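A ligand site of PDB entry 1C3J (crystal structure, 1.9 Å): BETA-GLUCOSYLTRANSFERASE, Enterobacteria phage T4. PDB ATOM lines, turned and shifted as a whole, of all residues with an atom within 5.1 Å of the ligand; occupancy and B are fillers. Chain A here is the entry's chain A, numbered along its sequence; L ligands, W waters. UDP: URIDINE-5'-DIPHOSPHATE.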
ATOM      1  N   VAL A  18      24.440  -3.621 -16.776  1.00  0.00           N
ATOM      2  CA  VAL A  18      24.072  -2.444 -17.595  1.00  0.00           C
ATOM      3  C   VAL A  18      23.752  -1.184 -16.752  1.00  0.00           C
ATOM      4  O   VAL A  18      24.161  -0.093 -17.116  1.00  0.00           O
ATOM      5  CB  VAL A  18      22.912  -2.743 -18.631  1.00  0.00           C
ATOM      6  CG1 VAL A  18      22.528  -1.490 -19.405  1.00  0.00           C
ATOM      7  CG2 VAL A  18      23.383  -3.785 -19.628  1.00  0.00           C
ATOM      8  N   ASP A 100      13.562   6.075 -18.627  1.00  0.00           N
ATOM      9  CA  ASP A 100      12.776   4.889 -18.946  1.00  0.00           C
ATOM     10  C   ASP A 100      11.364   5.100 -18.386  1.00  0.00           C
ATOM     11  O   ASP A 100      11.201   5.340 -17.202  1.00  0.00           O
ATOM     12  CB  ASP A 100      13.456   3.651 -18.331  1.00  0.00           C
ATOM     13  CG  ASP A 100      12.858   2.351 -18.795  1.00  0.00           C
ATOM     14  OD1 ASP A 100      11.615   2.233 -18.932  1.00  0.00           O
ATOM     15  OD2 ASP A 100      13.654   1.420 -19.000  1.00  0.00           O
ATOM     16  N   LYS A 166      26.155   9.063 -25.221  1.00  0.00           N
ATOM     17  CA  LYS A 166      27.027   8.124 -25.917  1.00  0.00           C
ATOM     18  C   LYS A 166      27.777   8.758 -27.078  1.00  0.00           C
ATOM     19  O   LYS A 166      28.998   8.671 -27.145  1.00  0.00           O
ATOM     20  CB  LYS A 166      26.232   6.890 -26.403  1.00  0.00           C
ATOM     21  CG  LYS A 166      27.130   5.640 -26.659  1.00  0.00           C
ATOM     22  CD  LYS A 166      26.301   4.333 -26.753  1.00  0.00           C
ATOM     23  CE  LYS A 166      27.061   3.110 -26.196  1.00  0.00           C
ATOM     24  NZ  LYS A 166      26.194   1.897 -25.970  1.00  0.00           N
ATOM     25  N   TYR A 186      18.341  -6.970 -33.450  1.00  0.00           N
ATOM     26  CA  TYR A 186      17.725  -6.134 -32.436  1.00  0.00           C
ATOM     27  C   TYR A 186      18.303  -6.607 -31.101  1.00  0.00           C
ATOM     28  O   TYR A 186      18.282  -7.794 -30.801  1.00  0.00           O
ATOM     29  CB  TYR A 186      16.216  -6.305 -32.441  1.00  0.00           C
ATOM     30  CG  TYR A 186      15.501  -5.556 -31.336  1.00  0.00           C
ATOM     31  CD1 TYR A 186      15.104  -4.245 -31.519  1.00  0.00           C
ATOM     32  CD2 TYR A 186      15.213  -6.171 -30.132  1.00  0.00           C
ATOM     33  CE1 TYR A 186      14.431  -3.539 -30.508  1.00  0.00           C
ATOM     34  CE2 TYR A 186      14.549  -5.477 -29.104  1.00  0.00           C
ATOM     35  CZ  TYR A 186      14.161  -4.167 -29.316  1.00  0.00           C
ATOM     36  OH  TYR A 186      13.530  -3.481 -28.333  1.00  0.00           O
ATOM     37  N   GLY A 187      18.814  -5.671 -30.323  1.00  0.00           N
ATOM     38  CA  GLY A 187      19.363  -6.047 -29.033  1.00  0.00           C
ATOM     39  C   GLY A 187      18.570  -5.391 -27.916  1.00  0.00           C
ATOM     40  O   GLY A 187      18.274  -4.203 -27.989  1.00  0.00           O
ATOM     41  N   GLY A 188      18.178  -6.161 -26.904  1.00  0.00           N
ATOM     42  CA  GLY A 188      17.460  -5.552 -25.805  1.00  0.00           C
ATOM     43  C   GLY A 188      16.854  -6.581 -24.907  1.00  0.00           C
ATOM     44  O   GLY A 188      17.106  -7.797 -25.066  1.00  0.00           O
ATOM     45  N   SER A 189      16.043  -6.129 -23.948  1.00  0.00           N
ATOM     46  CA  SER A 189      15.400  -7.068 -23.056  1.00  0.00           C
ATOM     47  C   SER A 189      13.886  -7.186 -23.346  1.00  0.00           C
ATOM     48  O   SER A 189      13.369  -6.522 -24.245  1.00  0.00           O
ATOM     49  CB  SER A 189      15.723  -6.707 -21.599  1.00  0.00           C
ATOM     50  OG  SER A 189      14.983  -5.590 -21.190  1.00  0.00           O
ATOM     51  N   ARG A 191      11.374  -6.354 -21.491  1.00  0.00           N
ATOM     52  CA  ARG A 191      10.646  -5.215 -20.899  1.00  0.00           C
ATOM     53  C   ARG A 191       9.276  -5.534 -20.329  1.00  0.00           C
ATOM     54  O   ARG A 191       8.341  -4.769 -20.516  1.00  0.00           O
ATOM     55  CB  ARG A 191      10.508  -4.051 -21.894  1.00  0.00           C
ATOM     56  CG  ARG A 191      11.831  -3.400 -22.305  1.00  0.00           C
ATOM     57  CD  ARG A 191      11.675  -2.198 -23.239  1.00  0.00           C
ATOM     58  NE  ARG A 191      10.912  -1.117 -22.619  1.00  0.00           N
ATOM     59  CZ  ARG A 191      11.388  -0.280 -21.701  1.00  0.00           C
ATOM     60  NH1 ARG A 191      12.646  -0.383 -21.297  1.00  0.00           N
ATOM     61  NH2 ARG A 191      10.614   0.655 -21.163  1.00  0.00           N
ATOM     62  N   ARG A 195       6.501  -4.400 -25.005  1.00  0.00           N
ATOM     63  CA  ARG A 195       6.718  -4.159 -26.430  1.00  0.00           C
ATOM     64  C   ARG A 195       6.523  -5.457 -27.228  1.00  0.00           C
ATOM     65  O   ARG A 195       6.932  -5.546 -28.397  1.00  0.00           O
ATOM     66  CB  ARG A 195       8.186  -3.701 -26.572  1.00  0.00           C
ATOM     67  CG  ARG A 195       8.536  -2.950 -27.762  1.00  0.00           C
ATOM     68  CD  ARG A 195       9.986  -2.528 -27.629  1.00  0.00           C
ATOM     69  NE  ARG A 195      10.152  -1.476 -26.610  1.00  0.00           N
ATOM     70  CZ  ARG A 195      11.253  -0.768 -26.425  1.00  0.00           C
ATOM     71  NH1 ARG A 195      12.339  -0.977 -27.187  1.00  0.00           N
ATOM     72  NH2 ARG A 195      11.233   0.245 -25.552  1.00  0.00           N
ATOM     73  N   PHE A 213      19.552 -10.148 -29.628  1.00  0.00           N
ATOM     74  CA  PHE A 213      20.534 -10.326 -28.548  1.00  0.00           C
ATOM     75  C   PHE A 213      20.066  -9.549 -27.329  1.00  0.00           C
ATOM     76  O   PHE A 213      19.219  -8.685 -27.468  1.00  0.00           O
ATOM     77  CB  PHE A 213      21.965  -9.927 -28.946  1.00  0.00           C
ATOM     78  CG  PHE A 213      22.153  -8.460 -29.249  1.00  0.00           C
ATOM     79  CD1 PHE A 213      21.845  -7.957 -30.499  1.00  0.00           C
ATOM     80  CD2 PHE A 213      22.743  -7.621 -28.319  1.00  0.00           C
ATOM     81  CE1 PHE A 213      22.121  -6.655 -30.834  1.00  0.00           C
ATOM     82  CE2 PHE A 213      23.035  -6.297 -28.628  1.00  0.00           C
ATOM     83  CZ  PHE A 213      22.725  -5.813 -29.903  1.00  0.00           C
ATOM     84  N   GLY A 214      20.593  -9.884 -26.141  1.00  0.00           N
ATOM     85  CA  GLY A 214      20.193  -9.206 -24.927  1.00  0.00           C
ATOM     86  C   GLY A 214      19.582 -10.160 -23.930  1.00  0.00           C
ATOM     87  O   GLY A 214      19.799 -11.362 -24.020  1.00  0.00           O
ATOM     88  N   GLY A 236      22.895 -14.283 -26.119  1.00  0.00           N
ATOM     89  CA  GLY A 236      23.033 -13.579 -24.852  1.00  0.00           C
ATOM     90  C   GLY A 236      23.364 -12.106 -24.839  1.00  0.00           C
ATOM     91  O   GLY A 236      23.529 -11.499 -25.894  1.00  0.00           O
ATOM     92  N   LYS A 237      23.459 -11.538 -23.644  1.00  0.00           N
ATOM     93  CA  LYS A 237      23.780 -10.122 -23.550  1.00  0.00           C
ATOM     94  C   LYS A 237      25.238  -9.892 -23.787  1.00  0.00           C
ATOM     95  O   LYS A 237      26.027 -10.813 -23.707  1.00  0.00           O
ATOM     96  CB  LYS A 237      23.331  -9.490 -22.232  1.00  0.00           C
ATOM     97  CG  LYS A 237      23.607 -10.261 -20.989  1.00  0.00           C
ATOM     98  CD  LYS A 237      22.864  -9.574 -19.832  1.00  0.00           C
ATOM     99  CE  LYS A 237      22.977 -10.310 -18.501  1.00  0.00           C
ATOM    100  NZ  LYS A 237      22.269  -9.545 -17.429  1.00  0.00           N
ATOM    101  N   ILE A 238      25.564  -8.684 -24.202  1.00  0.00           N
ATOM    102  CA  ILE A 238      26.918  -8.299 -24.478  1.00  0.00           C
ATOM    103  C   ILE A 238      27.099  -6.972 -23.766  1.00  0.00           C
ATOM    104  O   ILE A 238      26.110  -6.312 -23.401  1.00  0.00           O
ATOM    105  CB  ILE A 238      27.149  -8.108 -25.982  1.00  0.00           C
ATOM    106  CG1 ILE A 238      26.226  -7.032 -26.519  1.00  0.00           C
ATOM    107  CG2 ILE A 238      26.833  -9.389 -26.737  1.00  0.00           C
ATOM    108  CD1 ILE A 238      26.437  -6.795 -27.956  1.00  0.00           C
ATOM    109  N   PRO A 239      28.351  -6.582 -23.507  1.00  0.00           N
ATOM    110  CA  PRO A 239      28.579  -5.308 -22.814  1.00  0.00           C
ATOM    111  C   PRO A 239      28.053  -4.136 -23.625  1.00  0.00           C
ATOM    112  O   PRO A 239      28.110  -4.121 -24.856  1.00  0.00           O
ATOM    113  CB  PRO A 239      30.115  -5.247 -22.701  1.00  0.00           C
ATOM    114  CG  PRO A 239      30.518  -6.694 -22.686  1.00  0.00           C
ATOM    115  CD  PRO A 239      29.615  -7.313 -23.712  1.00  0.00           C
ATOM    116  N   MET A 240      27.678  -3.084 -22.912  1.00  0.00           N
ATOM    117  CA  MET A 240      27.167  -1.870 -23.515  1.00  0.00           C
ATOM    118  C   MET A 240      28.089  -1.281 -24.561  1.00  0.00           C
ATOM    119  O   MET A 240      27.641  -0.730 -25.559  1.00  0.00           O
ATOM    120  CB  MET A 240      26.946  -0.805 -22.445  1.00  0.00           C
ATOM    121  CG  MET A 240      25.524  -0.605 -22.031  1.00  0.00           C
ATOM    122  SD  MET A 240      25.423   0.971 -21.203  1.00  0.00           S
ATOM    123  CE  MET A 240      25.419   2.134 -22.585  1.00  0.00           C
ATOM    124  N   VAL A 243      27.756  -2.901 -28.293  1.00  0.00           N
ATOM    125  CA  VAL A 243      26.463  -2.900 -28.980  1.00  0.00           C
ATOM    126  C   VAL A 243      26.489  -2.458 -30.444  1.00  0.00           C
ATOM    127  O   VAL A 243      25.876  -3.116 -31.297  1.00  0.00           O
ATOM    128  CB  VAL A 243      25.388  -2.108 -28.197  1.00  0.00           C
ATOM    129  CG1 VAL A 243      24.117  -1.981 -29.012  1.00  0.00           C
ATOM    130  CG2 VAL A 243      25.048  -2.826 -26.917  1.00  0.00           C
ATOM    131  N   ILE A 256      12.234   0.139 -32.483  1.00  0.00           N
ATOM    132  CA  ILE A 256      10.829   0.065 -32.039  1.00  0.00           C
ATOM    133  C   ILE A 256      10.859   0.671 -30.606  1.00  0.00           C
ATOM    134  O   ILE A 256      11.936   0.975 -30.072  1.00  0.00           O
ATOM    135  CB  ILE A 256      10.250  -1.370 -31.991  1.00  0.00           C
ATOM    136  CG1 ILE A 256      11.240  -2.354 -31.402  1.00  0.00           C
ATOM    137  CG2 ILE A 256       9.860  -1.854 -33.415  1.00  0.00           C
ATOM    138  CD1 ILE A 256      10.610  -3.711 -31.130  1.00  0.00           C
ATOM    139  N   TYR A 261       6.705   5.951 -25.828  1.00  0.00           N
ATOM    140  CA  TYR A 261       7.945   6.484 -26.404  1.00  0.00           C
ATOM    141  C   TYR A 261       7.671   7.086 -27.778  1.00  0.00           C
ATOM    142  O   TYR A 261       8.459   7.900 -28.261  1.00  0.00           O
ATOM    143  CB  TYR A 261       8.994   5.387 -26.628  1.00  0.00           C
ATOM    144  CG  TYR A 261       9.680   4.943 -25.377  1.00  0.00           C
ATOM    145  CD1 TYR A 261       9.306   5.457 -24.135  1.00  0.00           C
ATOM    146  CD2 TYR A 261      10.711   4.001 -25.426  1.00  0.00           C
ATOM    147  CE1 TYR A 261       9.918   5.066 -22.982  1.00  0.00           C
ATOM    148  CE2 TYR A 261      11.339   3.585 -24.240  1.00  0.00           C
ATOM    149  CZ  TYR A 261      10.924   4.140 -23.025  1.00  0.00           C
ATOM    150  OH  TYR A 261      11.445   3.716 -21.828  1.00  0.00           O
ATOM    151  N   THR A 267      15.533   7.022 -28.135  1.00  0.00           N
ATOM    152  CA  THR A 267      16.223   6.142 -27.216  1.00  0.00           C
ATOM    153  C   THR A 267      17.699   5.949 -27.592  1.00  0.00           C
ATOM    154  O   THR A 267      18.113   6.260 -28.699  1.00  0.00           O
ATOM    155  CB  THR A 267      15.497   4.806 -27.168  1.00  0.00           C
ATOM    156  OG1 THR A 267      15.264   4.386 -28.514  1.00  0.00           O
ATOM    157  CG2 THR A 267      14.138   4.944 -26.443  1.00  0.00           C
ATOM    158  N   LEU A 268      18.489   5.403 -26.663  1.00  0.00           N
ATOM    159  CA  LEU A 268      19.916   5.181 -26.875  1.00  0.00           C
ATOM    160  C   LEU A 268      20.150   4.308 -28.108  1.00  0.00           C
ATOM    161  O   LEU A 268      21.093   4.552 -28.881  1.00  0.00           O
ATOM    162  CB  LEU A 268      20.555   4.549 -25.619  1.00  0.00           C
ATOM    163  CG  LEU A 268      22.067   4.287 -25.587  1.00  0.00           C
ATOM    164  CD1 LEU A 268      22.802   5.587 -25.905  1.00  0.00           C
ATOM    165  CD2 LEU A 268      22.500   3.727 -24.237  1.00  0.00           C
ATOM    166  N   ARG A 269      19.260   3.354 -28.338  1.00  0.00           N
ATOM    167  CA  ARG A 269      19.415   2.495 -29.498  1.00  0.00           C
ATOM    168  C   ARG A 269      19.408   3.273 -30.803  1.00  0.00           C
ATOM    169  O   ARG A 269      19.998   2.819 -31.774  1.00  0.00           O
ATOM    170  CB  ARG A 269      18.393   1.366 -29.541  1.00  0.00           C
ATOM    171  CG  ARG A 269      17.023   1.755 -29.985  1.00  0.00           C
ATOM    172  CD  ARG A 269      16.193   0.509 -30.230  1.00  0.00           C
ATOM    173  NE  ARG A 269      15.946  -0.257 -29.025  1.00  0.00           N
ATOM    174  CZ  ARG A 269      16.565  -1.403 -28.723  1.00  0.00           C
ATOM    175  NH1 ARG A 269      17.469  -1.931 -29.568  1.00  0.00           N
ATOM    176  NH2 ARG A 269      16.297  -2.027 -27.583  1.00  0.00           N
ATOM    177  N   GLU A 272      23.049   4.200 -31.096  1.00  0.00           N
ATOM    178  CA  GLU A 272      23.860   2.972 -31.180  1.00  0.00           C
ATOM    179  C   GLU A 272      23.711   2.375 -32.578  1.00  0.00           C
ATOM    180  O   GLU A 272      24.679   1.874 -33.168  1.00  0.00           O
ATOM    181  CB  GLU A 272      23.407   1.965 -30.156  1.00  0.00           C
ATOM    182  CG  GLU A 272      23.770   2.315 -28.722  1.00  0.00           C
ATOM    183  CD  GLU A 272      23.142   1.374 -27.713  1.00  0.00           C
ATOM    184  OE1 GLU A 272      22.048   0.787 -28.010  1.00  0.00           O
ATOM    185  OE2 GLU A 272      23.702   1.209 -26.608  1.00  0.00           O
HETATM  186  N1  UDP L   1      22.001  -3.561 -24.246  1.00  0.00           N
HETATM  187  C2  UDP L   1      23.246  -4.009 -23.831  1.00  0.00           C
HETATM  188  N3  UDP L   1      23.545  -5.328 -24.106  1.00  0.00           N
HETATM  189  C4  UDP L   1      22.727  -6.242 -24.758  1.00  0.00           C
HETATM  190  C5  UDP L   1      21.453  -5.707 -25.190  1.00  0.00           C
HETATM  191  C6  UDP L   1      21.121  -4.406 -24.919  1.00  0.00           C
HETATM  192  O2  UDP L   1      24.065  -3.256 -23.303  1.00  0.00           O
HETATM  193  O4  UDP L   1      23.087  -7.385 -24.893  1.00  0.00           O
HETATM  194  C1' UDP L   1      21.631  -2.193 -23.907  1.00  0.00           C
HETATM  195  C2' UDP L   1      21.837  -1.287 -25.085  1.00  0.00           C
HETATM  196  O2' UDP L   1      22.457  -0.049 -24.683  1.00  0.00           O
HETATM  197  C3' UDP L   1      20.435  -1.061 -25.579  1.00  0.00           C
HETATM  198  C4' UDP L   1      19.631  -1.160 -24.358  1.00  0.00           C
HETATM  199  O4' UDP L   1      20.257  -2.154 -23.573  1.00  0.00           O
HETATM  200  O3' UDP L   1      20.269   0.204 -26.212  1.00  0.00           O
HETATM  201  C5' UDP L   1      18.216  -1.544 -24.683  1.00  0.00           C
HETATM  202  O5' UDP L   1      17.378  -1.372 -23.557  1.00  0.00           O
HETATM  203  PA  UDP L   1      15.834  -1.831 -23.576  1.00  0.00           P
HETATM  204  O1A UDP L   1      15.233  -1.438 -22.268  1.00  0.00           O
HETATM  205  O2A UDP L   1      15.800  -3.261 -23.952  1.00  0.00           O
HETATM  206  O3A UDP L   1      15.176  -0.986 -24.792  1.00  0.00           O
HETATM  207  PB  UDP L   1      14.884   0.585 -25.081  1.00  0.00           P
HETATM  208  O1B UDP L   1      13.718   0.928 -24.248  1.00  0.00           O
HETATM  209  O2B UDP L   1      16.102   1.302 -24.732  1.00  0.00           O
HETATM  210  O3B UDP L   1      14.611   0.588 -26.516  1.00  0.00           O
HETATM  211  O   HOH W   1      18.113   2.161 -25.990  1.00  0.00           O
HETATM  212  O   HOH W   2      16.676   1.045 -21.511  1.00  0.00           O
HETATM  213  O   HOH W   3      21.184   1.099 -22.169  1.00  0.00           O
HETATM  214  O   HOH W   4      13.571   2.311 -28.311  1.00  0.00           O
HETATM  215  O   HOH W   5      13.777  -4.188 -25.833  1.00  0.00           O
HETATM  216  O   HOH W   6      13.813   2.479 -22.170  1.00  0.00           O
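OE1 of Glu 272 is in hydrogen-bond range of O3' of the ligand (2.6 Å).
An oxygen (O4) of the ligand is in hydrogen-bond range of the backbone NH of Ile 238 (2.9 Å).
O of Ile 238 sits at hydrogen-bond distance from N3 of the ligand, at 2.8 Å.
O3B of the ligand is in salt-bridge range of NH1 of Arg 195, 2.8 Å away.
An oxygen (O2A) of the ligand sits at hydrogen-bond distance from the backbone NH (N) of Ser 189, at 2.9 Å.
The guanidinium group (NH1) of Arg 191 lies within salt-bridge range of an oxygen (O1A) of the ligand.
An oxygen (O3B) of the ligand lies within salt-bridge range of the guanidinium group of Arg 269, 3.0 Å away.
The side-chain carboxylate (OE2) of Glu 272 is in salt-bridge range of the side-chain amino group (NZ) of Lys 166, at 2.7 Å.
OH of Tyr 186 lies within hydrogen-bond range of NH1 of Arg 195 (3.0 Å).
NH2 of Arg 191 sits at hydrogen-bond distance from OH of Tyr 261.
NH2 of Arg 191 lies within salt-bridge range of OD1 of Asp 100, 2.9 Å away.
The backbone carbonyl oxygen (O) of Met 240 sits at hydrogen-bond distance from the side-chain amino group (NZ) of Lys 166 (3.0 Å).
The backbone carbonyl oxygen (O) of Gly 236 is in hydrogen-bond range of the backbone NH (N) of Gly 214 (3.4 Å).
The backbone NH (N) of Phe 213 is in hydrogen-bond range of the backbone carbonyl oxygen (O) of Tyr 186, at 2.9 Å.
The side-chain hydroxyl (OH) of Tyr 261 lies within hydrogen-bond range of the side-chain carboxylate (OD1) of Asp 100, 3.3 Å away.
Val 18 touches the ligand.
Gly 187 touches the ligand.
Gly 188 touches the ligand.
Phe 213 touches the ligand.
Gly 214 touches the ligand (CA to O4, 3.4 Å).
Lys 237 touches the ligand (CA to O4, 3.1 Å).
Met 240 touches the ligand.
Val 243 touches the ligand.
CE2 of Tyr 261 touches O1B of the ligand, 3.6 Å away.
CD2 of Leu 268 touches O2' of the ligand, at 3.8 Å.
Hydrophobic or aromatic side chains that line the ligand: Val 18, Phe 213, Ile 238, Met 240, Val 243, Tyr 261 and Leu 268.
Water W1 lies within hydrogen-bond range of an oxygen (O2B) of the ligand (2.5 Å), the backbone NH of Arg 269 (2.9 Å) and the backbone NH of Leu 268 (3.3 Å).
Water W6 lies within hydrogen-bond range of O1B of the ligand (2.6 Å), OH of Tyr 261 (2.7 Å), NH1 of Arg 191 (3.2 Å) and OD2 of Asp 100 (3.3 Å).
Water W4 lies within hydrogen-bond range of the side-chain hydroxyl of Thr 267 (2.7 Å), an oxygen (O3B) of the ligand (2.7 Å) and the backbone carbonyl oxygen of Ile 256 (2.7 Å).
Water W5 lies within hydrogen-bond range of the side-chain hydroxyl of Tyr 186 (2.6 Å), the backbone carbonyl oxygen of Ser 189 (2.9 Å) and an oxygen (O2A) of the ligand (2.9 Å).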
